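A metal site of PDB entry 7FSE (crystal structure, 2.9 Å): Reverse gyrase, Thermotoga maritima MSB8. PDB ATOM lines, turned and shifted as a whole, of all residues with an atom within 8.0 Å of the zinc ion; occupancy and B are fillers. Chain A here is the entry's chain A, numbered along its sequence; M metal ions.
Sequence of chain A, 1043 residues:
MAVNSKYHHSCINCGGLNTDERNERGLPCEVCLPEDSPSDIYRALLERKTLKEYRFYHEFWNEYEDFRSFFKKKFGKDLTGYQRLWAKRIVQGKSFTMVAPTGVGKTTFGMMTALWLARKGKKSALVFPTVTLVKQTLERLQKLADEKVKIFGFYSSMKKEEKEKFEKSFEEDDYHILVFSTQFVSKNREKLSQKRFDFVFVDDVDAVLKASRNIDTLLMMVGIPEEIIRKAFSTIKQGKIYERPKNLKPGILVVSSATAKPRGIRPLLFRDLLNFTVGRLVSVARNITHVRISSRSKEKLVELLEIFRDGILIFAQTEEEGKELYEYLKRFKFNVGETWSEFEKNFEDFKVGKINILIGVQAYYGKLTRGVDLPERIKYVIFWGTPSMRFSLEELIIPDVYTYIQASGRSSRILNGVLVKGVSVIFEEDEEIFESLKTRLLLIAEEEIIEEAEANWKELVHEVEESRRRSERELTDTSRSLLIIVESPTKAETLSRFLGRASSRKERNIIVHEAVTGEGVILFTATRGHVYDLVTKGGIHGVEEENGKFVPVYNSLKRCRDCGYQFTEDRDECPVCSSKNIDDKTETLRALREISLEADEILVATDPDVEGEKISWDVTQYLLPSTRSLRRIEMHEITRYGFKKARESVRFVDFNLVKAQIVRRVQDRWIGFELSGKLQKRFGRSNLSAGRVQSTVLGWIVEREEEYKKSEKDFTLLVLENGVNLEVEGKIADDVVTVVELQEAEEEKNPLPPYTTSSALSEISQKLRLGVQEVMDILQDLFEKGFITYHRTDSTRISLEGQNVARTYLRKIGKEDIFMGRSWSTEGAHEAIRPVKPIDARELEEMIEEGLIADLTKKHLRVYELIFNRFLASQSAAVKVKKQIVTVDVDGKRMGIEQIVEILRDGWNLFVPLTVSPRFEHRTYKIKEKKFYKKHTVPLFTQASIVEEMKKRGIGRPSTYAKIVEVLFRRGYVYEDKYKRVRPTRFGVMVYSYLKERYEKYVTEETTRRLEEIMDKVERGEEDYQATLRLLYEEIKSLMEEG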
ATOM      1  N   ARG A 559      -8.480  14.447  15.892  1.00  0.00           N
ATOM      2  CA  ARG A 559      -7.591  15.603  15.889  1.00  0.00           C
ATOM      3  C   ARG A 559      -6.230  15.155  16.363  1.00  0.00           C
ATOM      4  O   ARG A 559      -6.093  14.626  17.478  1.00  0.00           O
ATOM      5  CB  ARG A 559      -8.137  16.722  16.773  1.00  0.00           C
ATOM      6  CG  ARG A 559      -7.331  18.008  16.715  1.00  0.00           C
ATOM      7  CD  ARG A 559      -7.806  19.022  17.740  1.00  0.00           C
ATOM      8  NE  ARG A 559      -7.643  18.529  19.107  1.00  0.00           N
ATOM      9  CZ  ARG A 559      -6.514  18.602  19.795  1.00  0.00           C
ATOM     10  NH1 ARG A 559      -5.416  19.145  19.278  1.00  0.00           N
ATOM     11  NH2 ARG A 559      -6.485  18.116  21.036  1.00  0.00           N
ATOM     12  N   CYS A 560      -5.216  15.357  15.527  1.00  0.00           N
ATOM     13  CA  CYS A 560      -3.845  15.053  15.936  1.00  0.00           C
ATOM     14  C   CYS A 560      -3.383  16.079  16.953  1.00  0.00           C
ATOM     15  O   CYS A 560      -3.496  17.292  16.738  1.00  0.00           O
ATOM     16  CB  CYS A 560      -2.927  15.054  14.711  1.00  0.00           C
ATOM     17  SG  CYS A 560      -1.185  14.802  15.080  1.00  0.00           S
ATOM     18  N   ARG A 561      -2.860  15.607  18.086  1.00  0.00           N
ATOM     19  CA  ARG A 561      -2.447  16.518  19.142  1.00  0.00           C
ATOM     20  C   ARG A 561      -1.137  17.223  18.830  1.00  0.00           C
ATOM     21  O   ARG A 561      -0.837  18.258  19.453  1.00  0.00           O
ATOM     22  CB  ARG A 561      -2.349  15.777  20.476  1.00  0.00           C
ATOM     23  CG  ARG A 561      -3.643  15.775  21.270  1.00  0.00           C
ATOM     24  CD  ARG A 561      -3.778  14.515  22.088  1.00  0.00           C
ATOM     25  NE  ARG A 561      -4.972  14.553  22.927  1.00  0.00           N
ATOM     26  CZ  ARG A 561      -5.612  13.478  23.359  1.00  0.00           C
ATOM     27  NH1 ARG A 561      -5.227  12.254  23.023  1.00  0.00           N
ATOM     28  NH2 ARG A 561      -6.692  13.628  24.130  1.00  0.00           N
ATOM     29  N   ASP A 562      -0.341  16.699  17.900  1.00  0.00           N
ATOM     30  CA  ASP A 562       0.963  17.272  17.591  1.00  0.00           C
ATOM     31  C   ASP A 562       0.876  18.357  16.516  1.00  0.00           C
ATOM     32  O   ASP A 562       1.246  19.506  16.768  1.00  0.00           O
ATOM     33  CB  ASP A 562       1.926  16.163  17.158  1.00  0.00           C
ATOM     34  CG  ASP A 562       2.233  15.189  18.279  1.00  0.00           C
ATOM     35  OD1 ASP A 562       1.806  15.456  19.429  1.00  0.00           O
ATOM     36  OD2 ASP A 562       2.899  14.165  18.019  1.00  0.00           O
ATOM     37  N   CYS A 563       0.397  18.004  15.335  1.00  0.00           N
ATOM     38  CA  CYS A 563       0.295  18.967  14.244  1.00  0.00           C
ATOM     39  C   CYS A 563      -1.088  19.582  14.100  1.00  0.00           C
ATOM     40  O   CYS A 563      -1.231  20.566  13.383  1.00  0.00           O
ATOM     41  CB  CYS A 563       0.705  18.327  12.912  1.00  0.00           C
ATOM     42  SG  CYS A 563      -0.550  17.265  12.171  1.00  0.00           S
ATOM     43  N   GLY A 564      -2.102  19.013  14.770  1.00  0.00           N
ATOM     44  CA  GLY A 564      -3.425  19.590  14.798  1.00  0.00           C
ATOM     45  C   GLY A 564      -4.318  19.273  13.625  1.00  0.00           C
ATOM     46  O   GLY A 564      -5.459  19.759  13.596  1.00  0.00           O
ATOM     47  N   TYR A 565      -3.862  18.484  12.661  1.00  0.00           N
ATOM     48  CA  TYR A 565      -4.687  18.149  11.509  1.00  0.00           C
ATOM     49  C   TYR A 565      -5.890  17.316  11.958  1.00  0.00           C
ATOM     50  O   TYR A 565      -5.772  16.441  12.818  1.00  0.00           O
ATOM     51  CB  TYR A 565      -3.871  17.395  10.469  1.00  0.00           C
ATOM     52  CG  TYR A 565      -4.633  17.059   9.209  1.00  0.00           C
ATOM     53  CD1 TYR A 565      -4.873  18.034   8.238  1.00  0.00           C
ATOM     54  CD2 TYR A 565      -5.121  15.777   8.979  1.00  0.00           C
ATOM     55  CE1 TYR A 565      -5.574  17.730   7.080  1.00  0.00           C
ATOM     56  CE2 TYR A 565      -5.822  15.472   7.821  1.00  0.00           C
ATOM     57  CZ  TYR A 565      -6.044  16.460   6.874  1.00  0.00           C
ATOM     58  OH  TYR A 565      -6.743  16.162   5.724  1.00  0.00           O
ATOM     59  N   GLN A 566      -7.039  17.588  11.356  1.00  0.00           N
ATOM     60  CA  GLN A 566      -8.274  16.893  11.665  1.00  0.00           C
ATOM     61  C   GLN A 566      -8.741  16.089  10.459  1.00  0.00           C
ATOM     62  O   GLN A 566      -8.619  16.531   9.315  1.00  0.00           O
ATOM     63  CB  GLN A 566      -9.364  17.864  12.099  1.00  0.00           C
ATOM     64  CG  GLN A 566      -9.102  18.508  13.449  1.00  0.00           C
ATOM     65  CD  GLN A 566     -10.254  19.370  13.921  1.00  0.00           C
ATOM     66  OE1 GLN A 566     -11.198  19.634  13.176  1.00  0.00           O
ATOM     67  NE2 GLN A 566     -10.192  19.799  15.172  1.00  0.00           N
ATOM     68  N   PHE A 567      -9.281  14.896  10.736  1.00  0.00           N
ATOM     69  CA  PHE A 567      -9.691  13.977   9.685  1.00  0.00           C
ATOM     70  C   PHE A 567     -10.798  13.081  10.222  1.00  0.00           C
ATOM     71  O   PHE A 567     -11.001  12.965  11.431  1.00  0.00           O
ATOM     72  CB  PHE A 567      -8.507  13.140   9.170  1.00  0.00           C
ATOM     73  CG  PHE A 567      -7.782  12.389  10.259  1.00  0.00           C
ATOM     74  CD1 PHE A 567      -6.867  13.035  11.072  1.00  0.00           C
ATOM     75  CD2 PHE A 567      -8.007  11.032  10.447  1.00  0.00           C
ATOM     76  CE1 PHE A 567      -6.198  12.346  12.062  1.00  0.00           C
ATOM     77  CE2 PHE A 567      -7.338  10.343  11.437  1.00  0.00           C
ATOM     78  CZ  PHE A 567      -6.436  10.995  12.249  1.00  0.00           C
ATOM     79  N   GLU A 573      -2.897   6.423  12.860  1.00  0.00           N
ATOM     80  CA  GLU A 573      -1.919   7.488  12.891  1.00  0.00           C
ATOM     81  C   GLU A 573      -2.402   8.681  12.076  1.00  0.00           C
ATOM     82  O   GLU A 573      -3.303   8.564  11.230  1.00  0.00           O
ATOM     83  CB  GLU A 573      -0.558   7.015  12.364  1.00  0.00           C
ATOM     84  CG  GLU A 573      -0.524   6.710  10.858  1.00  0.00           C
ATOM     85  CD  GLU A 573      -1.107   5.353  10.505  1.00  0.00           C
ATOM     86  OE1 GLU A 573      -2.298   5.104  10.813  1.00  0.00           O
ATOM     87  OE2 GLU A 573      -0.378   4.533   9.921  1.00  0.00           O
ATOM     88  N   CYS A 574      -1.812   9.837  12.352  1.00  0.00           N
ATOM     89  CA  CYS A 574      -2.151  11.053  11.623  1.00  0.00           C
ATOM     90  C   CYS A 574      -1.765  10.905  10.154  1.00  0.00           C
ATOM     91  O   CYS A 574      -0.646  10.478   9.856  1.00  0.00           O
ATOM     92  CB  CYS A 574      -1.461  12.257  12.251  1.00  0.00           C
ATOM     93  SG  CYS A 574      -1.751  13.824  11.411  1.00  0.00           S
ATOM     94  N   PRO A 575      -2.643  11.256   9.217  1.00  0.00           N
ATOM     95  CA  PRO A 575      -2.318  11.122   7.794  1.00  0.00           C
ATOM     96  C   PRO A 575      -1.345  12.172   7.276  1.00  0.00           C
ATOM     97  O   PRO A 575      -0.941  12.088   6.105  1.00  0.00           O
ATOM     98  CB  PRO A 575      -3.686  11.259   7.112  1.00  0.00           C
ATOM     99  CG  PRO A 575      -4.463  12.126   8.038  1.00  0.00           C
ATOM    100  CD  PRO A 575      -4.025  11.742   9.425  1.00  0.00           C
ATOM    101  N   VAL A 576      -0.968  13.155   8.076  1.00  0.00           N
ATOM    102  CA  VAL A 576      -0.098  14.236   7.640  1.00  0.00           C
ATOM    103  C   VAL A 576       1.288  14.145   8.282  1.00  0.00           C
ATOM    104  O   VAL A 576       2.293  14.359   7.609  1.00  0.00           O
ATOM    105  CB  VAL A 576      -0.744  15.610   7.905  1.00  0.00           C
ATOM    106  CG1 VAL A 576       0.181  16.721   7.455  1.00  0.00           C
ATOM    107  CG2 VAL A 576      -2.073  15.706   7.191  1.00  0.00           C
ATOM    108  N   CYS A 577       1.349  13.841   9.579  1.00  0.00           N
ATOM    109  CA  CYS A 577       2.633  13.777  10.279  1.00  0.00           C
ATOM    110  C   CYS A 577       2.945  12.406  10.851  1.00  0.00           C
ATOM    111  O   CYS A 577       4.025  12.237  11.444  1.00  0.00           O
ATOM    112  CB  CYS A 577       2.662  14.819  11.404  1.00  0.00           C
ATOM    113  SG  CYS A 577       1.770  14.337  12.900  1.00  0.00           S
ATOM    114  N   SER A 578       2.045  11.435  10.711  1.00  0.00           N
ATOM    115  CA  SER A 578       2.220  10.036  11.109  1.00  0.00           C
ATOM    116  C   SER A 578       2.309   9.834  12.618  1.00  0.00           C
ATOM    117  O   SER A 578       2.628   8.724  13.072  1.00  0.00           O
ATOM    118  CB  SER A 578       3.451   9.407  10.442  1.00  0.00           C
ATOM    119  OG  SER A 578       3.366   9.488   9.040  1.00  0.00           O
ATOM    120  N   SER A 579       2.034  10.863  13.420  1.00  0.00           N
ATOM    121  CA  SER A 579       1.980  10.678  14.864  1.00  0.00           C
ATOM    122  C   SER A 579       0.742   9.888  15.249  1.00  0.00           C
ATOM    123  O   SER A 579      -0.277   9.917  14.555  1.00  0.00           O
ATOM    124  CB  SER A 579       1.993  12.024  15.581  1.00  0.00           C
ATOM    125  OG  SER A 579       1.862  11.866  16.986  1.00  0.00           O
ATOM    126  N   LYS A 580       0.828   9.165  16.362  1.00  0.00           N
ATOM    127  CA  LYS A 580      -0.291   8.389  16.874  1.00  0.00           C
ATOM    128  C   LYS A 580      -0.965   9.058  18.073  1.00  0.00           C
ATOM    129  O   LYS A 580      -1.851   8.449  18.687  1.00  0.00           O
ATOM    130  CB  LYS A 580       0.168   6.976  17.256  1.00  0.00           C
ATOM    131  CG  LYS A 580       0.823   6.212  16.124  1.00  0.00           C
ATOM    132  CD  LYS A 580       1.159   4.789  16.523  1.00  0.00           C
ATOM    133  CE  LYS A 580      -0.020   3.850  16.343  1.00  0.00           C
ATOM    134  NZ  LYS A 580      -0.272   3.533  14.912  1.00  0.00           N
ATOM    135  N   ASN A 581      -0.570  10.280  18.416  1.00  0.00           N
ATOM    136  CA  ASN A 581      -1.173  11.017  19.528  1.00  0.00           C
ATOM    137  C   ASN A 581      -2.419  11.719  19.003  1.00  0.00           C
ATOM    138  O   ASN A 581      -2.436  12.928  18.751  1.00  0.00           O
ATOM    139  CB  ASN A 581      -0.172  11.994  20.132  1.00  0.00           C
ATOM    140  CG  ASN A 581      -0.681  12.643  21.393  1.00  0.00           C
ATOM    141  OD1 ASN A 581      -1.589  12.132  22.053  1.00  0.00           O
ATOM    142  ND2 ASN A 581      -0.092  13.781  21.762  1.00  0.00           N
ATOM    143  N   ILE A 582      -3.484  10.947  18.855  1.00  0.00           N
ATOM    144  CA  ILE A 582      -4.721  11.390  18.206  1.00  0.00           C
ATOM    145  C   ILE A 582      -5.781  11.621  19.260  1.00  0.00           C
ATOM    146  O   ILE A 582      -5.979  10.782  20.153  1.00  0.00           O
ATOM    147  CB  ILE A 582      -5.201  10.370  17.151  1.00  0.00           C
ATOM    148  CG1 ILE A 582      -4.613  10.692  15.775  1.00  0.00           C
ATOM    149  CG2 ILE A 582      -6.715  10.328  17.069  1.00  0.00           C
ATOM    150  CD1 ILE A 582      -3.127  10.468  15.670  1.00  0.00           C
HETATM  151 ZN    ZN M   1      -0.439  15.054  12.893  1.00  0.00          ZN
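The zinc ion is bound by the side-chain sulfur of Cys 577 (2.3 Å), the side-chain sulfur of Cys 560 (2.3 Å), the side-chain sulfur of Cys 563 (2.3 Å) and the side-chain sulfur of Cys 574 (2.3 Å).
The zinc ion has four donor atoms within binding distance.
The backbone NH (N) of Cys 560 is in hydrogen-bond range of the backbone carbonyl oxygen (O) of Tyr 565 (3.0 Å).
N of Tyr 565 lies close to SG of Cys 563, at 3.6 Å.
The backbone NH (N) of Asp 562 lies close to the side-chain sulfur (SG) of Cys 560 (3.5 Å).
The side-chain sulfur (SG) of Cys 577 lies close to the backbone NH (N) of Ser 579 (3.5 Å).
SG of Cys 574 sits close to N of Val 576 (3.5 Å).
O of Ser 579 lies within hydrogen-bond range of N of Cys 574.
The nearest printed residue that does not touch the zinc ion is Gly 564 (4.7 Å).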
